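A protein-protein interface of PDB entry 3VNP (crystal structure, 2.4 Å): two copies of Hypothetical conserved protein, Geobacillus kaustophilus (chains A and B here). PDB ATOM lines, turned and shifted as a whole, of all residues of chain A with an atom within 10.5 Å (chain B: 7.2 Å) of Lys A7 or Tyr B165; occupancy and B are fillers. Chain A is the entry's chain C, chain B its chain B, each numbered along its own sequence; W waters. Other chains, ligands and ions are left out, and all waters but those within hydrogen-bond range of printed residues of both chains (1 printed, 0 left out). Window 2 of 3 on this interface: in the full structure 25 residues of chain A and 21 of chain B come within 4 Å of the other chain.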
ATOM      1  N   ILE A   3      -9.761 -10.357   4.668  1.00  0.00           N
ATOM      2  CA  ILE A   3      -9.293  -9.871   3.372  1.00  0.00           C
ATOM      3  C   ILE A   3     -10.302  -8.829   2.909  1.00  0.00           C
ATOM      4  O   ILE A   3     -11.503  -9.077   2.906  1.00  0.00           O
ATOM      5  CB  ILE A   3      -9.222 -10.976   2.294  1.00  0.00           C
ATOM      6  CG1 ILE A   3      -8.251 -12.082   2.715  1.00  0.00           C
ATOM      7  CG2 ILE A   3      -8.765 -10.361   0.969  1.00  0.00           C
ATOM      8  CD1 ILE A   3      -6.796 -11.645   2.781  1.00  0.00           C
ATOM      9  N   TYR A   4      -9.818  -7.653   2.537  1.00  0.00           N
ATOM     10  CA  TYR A   4     -10.702  -6.596   2.087  1.00  0.00           C
ATOM     11  C   TYR A   4     -10.210  -5.954   0.810  1.00  0.00           C
ATOM     12  O   TYR A   4      -9.011  -5.800   0.602  1.00  0.00           O
ATOM     13  CB  TYR A   4     -10.813  -5.506   3.148  1.00  0.00           C
ATOM     14  CG  TYR A   4     -11.791  -5.777   4.259  1.00  0.00           C
ATOM     15  CD1 TYR A   4     -13.152  -5.923   3.995  1.00  0.00           C
ATOM     16  CD2 TYR A   4     -11.367  -5.830   5.585  1.00  0.00           C
ATOM     17  CE1 TYR A   4     -14.071  -6.106   5.027  1.00  0.00           C
ATOM     18  CE2 TYR A   4     -12.274  -6.014   6.621  1.00  0.00           C
ATOM     19  CZ  TYR A   4     -13.626  -6.147   6.336  1.00  0.00           C
ATOM     20  OH  TYR A   4     -14.525  -6.298   7.361  1.00  0.00           O
ATOM     21  N   PRO A   5     -11.136  -5.579  -0.074  1.00  0.00           N
ATOM     22  CA  PRO A   5     -10.719  -4.939  -1.318  1.00  0.00           C
ATOM     23  C   PRO A   5     -10.691  -3.445  -1.033  1.00  0.00           C
ATOM     24  O   PRO A   5     -11.128  -3.006   0.030  1.00  0.00           O
ATOM     25  CB  PRO A   5     -11.837  -5.305  -2.277  1.00  0.00           C
ATOM     26  CG  PRO A   5     -13.039  -5.211  -1.387  1.00  0.00           C
ATOM     27  CD  PRO A   5     -12.572  -5.909  -0.112  1.00  0.00           C
ATOM     28  N   TYR A   6     -10.157  -2.674  -1.965  1.00  0.00           N
ATOM     29  CA  TYR A   6     -10.131  -1.230  -1.813  1.00  0.00           C
ATOM     30  C   TYR A   6     -10.151  -0.553  -3.175  1.00  0.00           C
ATOM     31  O   TYR A   6      -9.183  -0.630  -3.932  1.00  0.00           O
ATOM     32  CB  TYR A   6      -8.899  -0.757  -1.044  1.00  0.00           C
ATOM     33  CG  TYR A   6      -9.016   0.703  -0.675  1.00  0.00           C
ATOM     34  CD1 TYR A   6      -9.858   1.109   0.360  1.00  0.00           C
ATOM     35  CD2 TYR A   6      -8.366   1.686  -1.418  1.00  0.00           C
ATOM     36  CE1 TYR A   6     -10.058   2.450   0.638  1.00  0.00           C
ATOM     37  CE2 TYR A   6      -8.558   3.038  -1.142  1.00  0.00           C
ATOM     38  CZ  TYR A   6      -9.409   3.408  -0.117  1.00  0.00           C
ATOM     39  OH  TYR A   6      -9.634   4.740   0.141  1.00  0.00           O
ATOM     40  N   LYS A   7     -11.264   0.104  -3.479  1.00  0.00           N
ATOM     41  CA  LYS A   7     -11.419   0.814  -4.740  1.00  0.00           C
ATOM     42  C   LYS A   7     -11.082  -0.070  -5.935  1.00  0.00           C
ATOM     43  O   LYS A   7     -10.346   0.344  -6.834  1.00  0.00           O
ATOM     44  CB  LYS A   7     -10.518   2.051  -4.774  1.00  0.00           C
ATOM     45  CG  LYS A   7     -10.648   2.988  -3.588  1.00  0.00           C
ATOM     46  CD  LYS A   7     -11.978   3.710  -3.536  1.00  0.00           C
ATOM     47  CE  LYS A   7     -11.947   4.779  -2.445  1.00  0.00           C
ATOM     48  NZ  LYS A   7     -13.210   5.561  -2.355  1.00  0.00           N
ATOM     49  N   GLY A   8     -11.606  -1.292  -5.932  1.00  0.00           N
ATOM     50  CA  GLY A   8     -11.370  -2.199  -7.040  1.00  0.00           C
ATOM     51  C   GLY A   8     -10.087  -3.002  -7.017  1.00  0.00           C
ATOM     52  O   GLY A   8      -9.740  -3.630  -8.014  1.00  0.00           O
ATOM     53  N   LYS A   9      -9.378  -2.989  -5.894  1.00  0.00           N
ATOM     54  CA  LYS A   9      -8.128  -3.740  -5.775  1.00  0.00           C
ATOM     55  C   LYS A   9      -8.257  -4.769  -4.668  1.00  0.00           C
ATOM     56  O   LYS A   9      -8.757  -4.452  -3.591  1.00  0.00           O
ATOM     57  CB  LYS A   9      -6.970  -2.815  -5.416  1.00  0.00           C
ATOM     58  CG  LYS A   9      -6.753  -1.648  -6.345  1.00  0.00           C
ATOM     59  CD  LYS A   9      -6.082  -2.070  -7.625  1.00  0.00           C
ATOM     60  CE  LYS A   9      -5.422  -0.860  -8.257  1.00  0.00           C
ATOM     61  NZ  LYS A   9      -6.375   0.287  -8.332  1.00  0.00           N
ATOM     62  N   THR A  10      -7.813  -5.996  -4.932  1.00  0.00           N
ATOM     63  CA  THR A  10      -7.853  -7.055  -3.929  1.00  0.00           C
ATOM     64  C   THR A  10      -6.501  -7.744  -3.863  1.00  0.00           C
ATOM     65  O   THR A  10      -5.758  -7.791  -4.848  1.00  0.00           O
ATOM     66  CB  THR A  10      -8.918  -8.126  -4.238  1.00  0.00           C
ATOM     67  OG1 THR A  10      -9.312  -8.020  -5.607  1.00  0.00           O
ATOM     68  CG2 THR A  10     -10.130  -7.957  -3.338  1.00  0.00           C
ATOM     69  N   PRO A  11      -6.154  -8.282  -2.691  1.00  0.00           N
ATOM     70  CA  PRO A  11      -4.868  -8.964  -2.545  1.00  0.00           C
ATOM     71  C   PRO A  11      -4.722 -10.188  -3.451  1.00  0.00           C
ATOM     72  O   PRO A  11      -5.690 -10.894  -3.702  1.00  0.00           O
ATOM     73  CB  PRO A  11      -4.852  -9.350  -1.068  1.00  0.00           C
ATOM     74  CG  PRO A  11      -5.639  -8.248  -0.423  1.00  0.00           C
ATOM     75  CD  PRO A  11      -6.792  -8.062  -1.382  1.00  0.00           C
ATOM     76  N   THR A  26      -5.585  -5.925   2.942  1.00  0.00           N
ATOM     77  CA  THR A  26      -6.581  -5.255   2.120  1.00  0.00           C
ATOM     78  C   THR A  26      -5.957  -4.534   0.943  1.00  0.00           C
ATOM     79  O   THR A  26      -4.761  -4.233   0.944  1.00  0.00           O
ATOM     80  CB  THR A  26      -7.376  -4.195   2.927  1.00  0.00           C
ATOM     81  OG1 THR A  26      -6.574  -3.013   3.067  1.00  0.00           O
ATOM     82  CG2 THR A  26      -7.736  -4.719   4.317  1.00  0.00           C
ATOM     83  N   GLY A  27      -6.785  -4.261  -0.060  1.00  0.00           N
ATOM     84  CA  GLY A  27      -6.345  -3.527  -1.230  1.00  0.00           C
ATOM     85  C   GLY A  27      -5.300  -4.115  -2.157  1.00  0.00           C
ATOM     86  O   GLY A  27      -5.205  -5.324  -2.349  1.00  0.00           O
ATOM     87  N   ASP A  28      -4.511  -3.217  -2.736  1.00  0.00           N
ATOM     88  CA  ASP A  28      -3.473  -3.561  -3.696  1.00  0.00           C
ATOM     89  C   ASP A  28      -2.257  -4.227  -3.053  1.00  0.00           C
ATOM     90  O   ASP A  28      -1.215  -3.597  -2.859  1.00  0.00           O
ATOM     91  CB  ASP A  28      -3.061  -2.290  -4.439  1.00  0.00           C
ATOM     92  CG  ASP A  28      -2.220  -2.572  -5.663  1.00  0.00           C
ATOM     93  OD1 ASP A  28      -2.036  -3.764  -6.009  1.00  0.00           O
ATOM     94  OD2 ASP A  28      -1.748  -1.594  -6.284  1.00  0.00           O
ATOM     95  N   ARG A  44      -2.343  -2.932   4.968  1.00  0.00           N
ATOM     96  CA  ARG A  44      -3.361  -2.150   4.276  1.00  0.00           C
ATOM     97  C   ARG A  44      -2.772  -1.539   3.021  1.00  0.00           C
ATOM     98  O   ARG A  44      -1.919  -0.656   3.098  1.00  0.00           O
ATOM     99  CB  ARG A  44      -3.906  -1.040   5.182  1.00  0.00           C
ATOM    100  CG  ARG A  44      -5.030  -1.480   6.116  1.00  0.00           C
ATOM    101  CD  ARG A  44      -5.365  -0.384   7.101  1.00  0.00           C
ATOM    102  NE  ARG A  44      -5.515   0.885   6.408  1.00  0.00           N
ATOM    103  CZ  ARG A  44      -5.246   2.071   6.939  1.00  0.00           C
ATOM    104  NH1 ARG A  44      -4.810   2.172   8.187  1.00  0.00           N
ATOM    105  NH2 ARG A  44      -5.398   3.159   6.204  1.00  0.00           N
ATOM    106  N   GLY A  45      -3.216  -2.022   1.866  1.00  0.00           N
ATOM    107  CA  GLY A  45      -2.718  -1.494   0.605  1.00  0.00           C
ATOM    108  C   GLY A  45      -3.782  -0.590   0.019  1.00  0.00           C
ATOM    109  O   GLY A  45      -4.317  -0.869  -1.054  1.00  0.00           O
ATOM    110  N   ASP A  46      -4.079   0.496   0.730  1.00  0.00           N
ATOM    111  CA  ASP A  46      -5.111   1.440   0.322  1.00  0.00           C
ATOM    112  C   ASP A  46      -4.600   2.845  -0.007  1.00  0.00           C
ATOM    113  O   ASP A  46      -5.376   3.796  -0.060  1.00  0.00           O
ATOM    114  CB  ASP A  46      -6.190   1.508   1.418  1.00  0.00           C
ATOM    115  CG  ASP A  46      -5.630   1.925   2.780  1.00  0.00           C
ATOM    116  OD1 ASP A  46      -6.298   1.665   3.813  1.00  0.00           O
ATOM    117  OD2 ASP A  46      -4.529   2.520   2.816  1.00  0.00           O
ATOM    118  N   VAL A  47      -3.295   2.971  -0.224  1.00  0.00           N
ATOM    119  CA  VAL A  47      -2.695   4.259  -0.557  1.00  0.00           C
ATOM    120  C   VAL A  47      -1.778   4.113  -1.772  1.00  0.00           C
ATOM    121  O   VAL A  47      -1.803   4.941  -2.684  1.00  0.00           O
ATOM    122  CB  VAL A  47      -1.885   4.827   0.636  1.00  0.00           C
ATOM    123  CG1 VAL A  47      -1.089   6.054   0.201  1.00  0.00           C
ATOM    124  CG2 VAL A  47      -2.830   5.183   1.786  1.00  0.00           C
ATOM    125  N   ALA A  48      -0.980   3.050  -1.782  1.00  0.00           N
ATOM    126  CA  ALA A  48      -0.054   2.774  -2.877  1.00  0.00           C
ATOM    127  C   ALA A  48       0.201   1.266  -2.932  1.00  0.00           C
ATOM    128  O   ALA A  48      -0.072   0.545  -1.975  1.00  0.00           O
ATOM    129  CB  ALA A  48       1.253   3.533  -2.667  1.00  0.00           C
ATOM    130  N   PHE B  18     -16.524   4.260  12.574  1.00  0.00           N
ATOM    131  CA  PHE B  18     -16.099   3.009  11.971  1.00  0.00           C
ATOM    132  C   PHE B  18     -15.200   2.267  12.961  1.00  0.00           C
ATOM    133  O   PHE B  18     -14.201   2.806  13.436  1.00  0.00           O
ATOM    134  CB  PHE B  18     -15.345   3.265  10.657  1.00  0.00           C
ATOM    135  CG  PHE B  18     -14.518   2.092  10.189  1.00  0.00           C
ATOM    136  CD1 PHE B  18     -15.106   0.859   9.943  1.00  0.00           C
ATOM    137  CD2 PHE B  18     -13.140   2.219  10.021  1.00  0.00           C
ATOM    138  CE1 PHE B  18     -14.332  -0.235   9.540  1.00  0.00           C
ATOM    139  CE2 PHE B  18     -12.357   1.133   9.619  1.00  0.00           C
ATOM    140  CZ  PHE B  18     -12.952  -0.095   9.378  1.00  0.00           C
ATOM    141  N   TRP B  38      -8.969   1.892  13.705  1.00  0.00           N
ATOM    142  CA  TRP B  38      -8.447   0.864  12.824  1.00  0.00           C
ATOM    143  C   TRP B  38      -8.003  -0.459  13.423  1.00  0.00           C
ATOM    144  O   TRP B  38      -7.809  -0.588  14.630  1.00  0.00           O
ATOM    145  CB  TRP B  38      -7.357   1.486  11.964  1.00  0.00           C
ATOM    146  CG  TRP B  38      -7.939   2.625  11.222  1.00  0.00           C
ATOM    147  CD1 TRP B  38      -8.197   3.879  11.712  1.00  0.00           C
ATOM    148  CD2 TRP B  38      -8.502   2.584   9.916  1.00  0.00           C
ATOM    149  NE1 TRP B  38      -8.896   4.615  10.789  1.00  0.00           N
ATOM    150  CE2 TRP B  38      -9.099   3.845   9.675  1.00  0.00           C
ATOM    151  CE3 TRP B  38      -8.572   1.600   8.923  1.00  0.00           C
ATOM    152  CZ2 TRP B  38      -9.752   4.150   8.482  1.00  0.00           C
ATOM    153  CZ3 TRP B  38      -9.226   1.902   7.732  1.00  0.00           C
ATOM    154  CH2 TRP B  38      -9.808   3.170   7.525  1.00  0.00           C
ATOM    155  N   TYR B 159      -8.975   9.967   6.009  1.00  0.00           N
ATOM    156  CA  TYR B 159      -9.349   8.933   6.959  1.00  0.00           C
ATOM    157  C   TYR B 159     -10.825   8.943   7.307  1.00  0.00           C
ATOM    158  O   TYR B 159     -11.400   7.885   7.591  1.00  0.00           O
ATOM    159  CB  TYR B 159      -8.484   9.003   8.218  1.00  0.00           C
ATOM    160  CG  TYR B 159      -7.266   8.121   8.093  1.00  0.00           C
ATOM    161  CD1 TYR B 159      -6.070   8.611   7.574  1.00  0.00           C
ATOM    162  CD2 TYR B 159      -7.336   6.765   8.415  1.00  0.00           C
ATOM    163  CE1 TYR B 159      -4.972   7.768   7.379  1.00  0.00           C
ATOM    164  CE2 TYR B 159      -6.254   5.916   8.223  1.00  0.00           C
ATOM    165  CZ  TYR B 159      -5.073   6.418   7.706  1.00  0.00           C
ATOM    166  OH  TYR B 159      -3.997   5.572   7.522  1.00  0.00           O
ATOM    167  N   VAL B 160     -11.444  10.123   7.286  1.00  0.00           N
ATOM    168  CA  VAL B 160     -12.869  10.197   7.563  1.00  0.00           C
ATOM    169  C   VAL B 160     -13.564   9.449   6.427  1.00  0.00           C
ATOM    170  O   VAL B 160     -14.504   8.685   6.662  1.00  0.00           O
ATOM    171  CB  VAL B 160     -13.389  11.663   7.610  1.00  0.00           C
ATOM    172  CG1 VAL B 160     -14.908  11.689   7.442  1.00  0.00           C
ATOM    173  CG2 VAL B 160     -13.029  12.299   8.941  1.00  0.00           C
ATOM    174  N   GLU B 161     -13.084   9.660   5.199  1.00  0.00           N
ATOM    175  CA  GLU B 161     -13.656   9.007   4.022  1.00  0.00           C
ATOM    176  C   GLU B 161     -13.295   7.525   3.950  1.00  0.00           C
ATOM    177  O   GLU B 161     -14.131   6.691   3.606  1.00  0.00           O
ATOM    178  CB  GLU B 161     -13.186   9.704   2.738  1.00  0.00           C
ATOM    179  CG  GLU B 161     -13.534  11.195   2.647  1.00  0.00           C
ATOM    180  CD  GLU B 161     -15.041  11.470   2.626  1.00  0.00           C
ATOM    181  OE1 GLU B 161     -15.726  10.987   1.692  1.00  0.00           O
ATOM    182  OE2 GLU B 161     -15.537  12.174   3.544  1.00  0.00           O
ATOM    183  N   LYS B 162     -12.050   7.198   4.280  1.00  0.00           N
ATOM    184  CA  LYS B 162     -11.590   5.815   4.244  1.00  0.00           C
ATOM    185  C   LYS B 162     -12.322   4.963   5.281  1.00  0.00           C
ATOM    186  O   LYS B 162     -12.634   3.790   5.033  1.00  0.00           O
ATOM    187  CB  LYS B 162     -10.084   5.755   4.495  1.00  0.00           C
ATOM    188  CG  LYS B 162      -9.446   4.475   4.019  1.00  0.00           C
ATOM    189  CD  LYS B 162      -7.985   4.380   4.435  1.00  0.00           C
ATOM    190  CE  LYS B 162      -7.110   5.454   3.779  1.00  0.00           C
ATOM    191  NZ  LYS B 162      -6.998   5.309   2.297  1.00  0.00           N
ATOM    192  N   GLY B 163     -12.585   5.556   6.446  1.00  0.00           N
ATOM    193  CA  GLY B 163     -13.292   4.846   7.495  1.00  0.00           C
ATOM    194  C   GLY B 163     -14.704   4.520   7.043  1.00  0.00           C
ATOM    195  O   GLY B 163     -15.205   3.421   7.298  1.00  0.00           O
ATOM    196  N   GLN B 164     -15.349   5.467   6.365  1.00  0.00           N
ATOM    197  CA  GLN B 164     -16.708   5.260   5.875  1.00  0.00           C
ATOM    198  C   GLN B 164     -16.722   4.233   4.752  1.00  0.00           C
ATOM    199  O   GLN B 164     -17.692   3.491   4.588  1.00  0.00           O
ATOM    200  CB  GLN B 164     -17.319   6.583   5.393  1.00  0.00           C
ATOM    201  CG  GLN B 164     -17.570   7.583   6.524  1.00  0.00           C
ATOM    202  CD  GLN B 164     -18.451   7.006   7.629  1.00  0.00           C
ATOM    203  OE1 GLN B 164     -19.633   6.740   7.418  1.00  0.00           O
ATOM    204  NE2 GLN B 164     -17.872   6.800   8.807  1.00  0.00           N
ATOM    205  N   TYR B 165     -15.641   4.183   3.984  1.00  0.00           N
ATOM    206  CA  TYR B 165     -15.549   3.230   2.891  1.00  0.00           C
ATOM    207  C   TYR B 165     -15.436   1.816   3.460  1.00  0.00           C
ATOM    208  O   TYR B 165     -16.158   0.906   3.041  1.00  0.00           O
ATOM    209  CB  TYR B 165     -14.329   3.525   2.024  1.00  0.00           C
ATOM    210  CG  TYR B 165     -14.236   2.614   0.828  1.00  0.00           C
ATOM    211  CD1 TYR B 165     -14.902   2.917  -0.357  1.00  0.00           C
ATOM    212  CD2 TYR B 165     -13.500   1.428   0.890  1.00  0.00           C
ATOM    213  CE1 TYR B 165     -14.838   2.068  -1.450  1.00  0.00           C
ATOM    214  CE2 TYR B 165     -13.430   0.572  -0.196  1.00  0.00           C
ATOM    215  CZ  TYR B 165     -14.099   0.899  -1.363  1.00  0.00           C
ATOM    216  OH  TYR B 165     -14.023   0.054  -2.443  1.00  0.00           O
ATOM    217  N   TYR B 166     -14.520   1.636   4.408  1.00  0.00           N
ATOM    218  CA  TYR B 166     -14.333   0.341   5.053  1.00  0.00           C
ATOM    219  C   TYR B 166     -15.573  -0.034   5.854  1.00  0.00           C
ATOM    220  O   TYR B 166     -15.932  -1.207   5.932  1.00  0.00           O
ATOM    221  CB  TYR B 166     -13.121   0.376   5.982  1.00  0.00           C
ATOM    222  CG  TYR B 166     -11.812   0.146   5.281  1.00  0.00           C
ATOM    223  CD1 TYR B 166     -11.374  -1.146   4.995  1.00  0.00           C
ATOM    224  CD2 TYR B 166     -10.999   1.213   4.915  1.00  0.00           C
ATOM    225  CE1 TYR B 166     -10.154  -1.371   4.367  1.00  0.00           C
ATOM    226  CE2 TYR B 166      -9.772   0.996   4.282  1.00  0.00           C
ATOM    227  CZ  TYR B 166      -9.356  -0.297   4.018  1.00  0.00           C
ATOM    228  OH  TYR B 166      -8.123  -0.517   3.451  1.00  0.00           O
ATOM    229  N   LYS B 167     -16.222   0.964   6.453  1.00  0.00           N
ATOM    230  CA  LYS B 167     -17.432   0.718   7.242  1.00  0.00           C
ATOM    231  C   LYS B 167     -18.491   0.036   6.374  1.00  0.00           C
ATOM    232  O   LYS B 167     -19.141  -0.914   6.800  1.00  0.00           O
ATOM    233  CB  LYS B 167     -17.981   2.039   7.798  1.00  0.00           C
ATOM    234  CG  LYS B 167     -19.193   1.909   8.728  1.00  0.00           C
ATOM    235  CD  LYS B 167     -19.458   3.256   9.417  1.00  0.00           C
ATOM    236  CE  LYS B 167     -20.804   3.332  10.129  1.00  0.00           C
ATOM    237  NZ  LYS B 167     -20.899   2.415  11.281  1.00  0.00           N
ATOM    238  N   ALA B 168     -18.645   0.523   5.147  1.00  0.00           N
ATOM    239  CA  ALA B 168     -19.618  -0.040   4.225  1.00  0.00           C
ATOM    240  C   ALA B 168     -19.253  -1.483   3.860  1.00  0.00           C
ATOM    241  O   ALA B 168     -20.118  -2.362   3.822  1.00  0.00           O
ATOM    242  CB  ALA B 168     -19.701   0.821   2.977  1.00  0.00           C
ATOM    243  N   LEU B 169     -17.976  -1.734   3.593  1.00  0.00           N
ATOM    244  CA  LEU B 169     -17.547  -3.085   3.249  1.00  0.00           C
ATOM    245  C   LEU B 169     -17.840  -4.017   4.414  1.00  0.00           C
ATOM    246  O   LEU B 169     -18.238  -5.162   4.224  1.00  0.00           O
ATOM    247  CB  LEU B 169     -16.047  -3.126   2.949  1.00  0.00           C
ATOM    248  CG  LEU B 169     -15.509  -2.350   1.745  1.00  0.00           C
ATOM    249  CD1 LEU B 169     -13.994  -2.430   1.744  1.00  0.00           C
ATOM    250  CD2 LEU B 169     -16.080  -2.916   0.452  1.00  0.00           C
ATOM    251  N   GLN B 170     -17.639  -3.517   5.626  1.00  0.00           N
ATOM    252  CA  GLN B 170     -17.862  -4.312   6.820  1.00  0.00           C
ATOM    253  C   GLN B 170     -19.289  -4.865   6.849  1.00  0.00           C
ATOM    254  O   GLN B 170     -19.506  -6.022   7.205  1.00  0.00           O
ATOM    255  CB  GLN B 170     -17.587  -3.458   8.054  1.00  0.00           C
ATOM    256  CG  GLN B 170     -17.094  -4.237   9.248  1.00  0.00           C
ATOM    257  CD  GLN B 170     -16.720  -3.330  10.402  1.00  0.00           C
ATOM    258  OE1 GLN B 170     -17.492  -2.450  10.783  1.00  0.00           O
ATOM    259  NE2 GLN B 170     -15.536  -3.541  10.968  1.00  0.00           N
HETATM  260  O   HOH W   1     -13.416  -2.285  -3.833  1.00  0.00           O
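The side-chain hydroxyl (OH) of Tyr B159 lies within hydrogen-bond range of the guanidinium group (NH2) of Arg A44 (3.1 Å).
The side-chain amino group (NZ) of Lys B162 lies within hydrogen-bond range of the side-chain hydroxyl (OH) of Tyr A6.
The side-chain amino group (NZ) of Lys B162 lies within salt-bridge range of the side-chain carboxylate (OD2) of Asp A46, 3.8 Å away.
The side-chain hydroxyl of Tyr B165 sits at hydrogen-bond distance from the backbone NH of Lys A7, 2.9 Å away.
The side-chain hydroxyl of Tyr B166 is in hydrogen-bond range of the side-chain hydroxyl of Thr A26, 3.0 Å away.
The side-chain hydroxyl (OH) of Tyr B166 lies within hydrogen-bond range of the side-chain carboxylate (OD1) of Asp A46.
Hydrophobic or aromatic side chains of chain B that line the printed part of chain A: Trp B38, Tyr B159, Tyr B165, Tyr B166 and Leu B169.
Of the 17 printed residues of chain A, 7 touch a printed residue of chain B.
Hydrophobic or aromatic side chains of chain A within 4 Å of the printed part of chain B: Tyr A4 and Tyr A6.
Printed residues of chain B within 4 Å of Tyr A4: Gln B170.
Of the printed residues of chain B, Pro A5 touches Leu B169 (3.4 Å).
Of the printed residues of chain B, Tyr A6 touches Lys B162, Tyr B165 and Tyr B166.
Val A47 touches none of the printed residues of chain B.
No residue of chain A comes within 4 Å of Gly B163.
No residue of chain A comes within 4 Å of Gln B164.
Tyr B165 touches just these residues of chain A: Tyr A6 and Lys A7.
Tyr B166 touches three residues of chain A.
Printed residues of chain A within 4 Å of Leu B169: Pro A5.
The nearest residue of chain B that does not touch Lys A7 is Glu B161 (6.1 Å).
The nearest residue of chain A that does not touch Tyr B165 is Pro A5 (4.3 Å).
O of Tyr A4 is in hydrogen-bond range of N of Gly A27 (2.8 Å).
O of Thr A26 lies within hydrogen-bond range of N of Gly A45.
NE of Arg A44 lies within salt-bridge range of OD1 of Asp A46 (2.8 Å).
Among the printed residues, merely in contact across the chains: Tyr A4 with Gln B170, Pro A5 with Leu B169, Tyr A6 with Tyr B165, Tyr A6 with Tyr B166, Arg A44 with Trp B38 and Arg A44 with Lys B162.
Water W1 lies within hydrogen-bond range of the side-chain hydroxyl (OH) of Tyr B165 (2.8 Å), the backbone NH (N) of Gly A8 (2.9 Å) and the backbone NH (N) of Lys A7 (3.2 Å).
No position is printed for both chains.
Of the 12 pairs that touch across the chains among the printed residues, none has its exchanged pair printed and touching as well.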
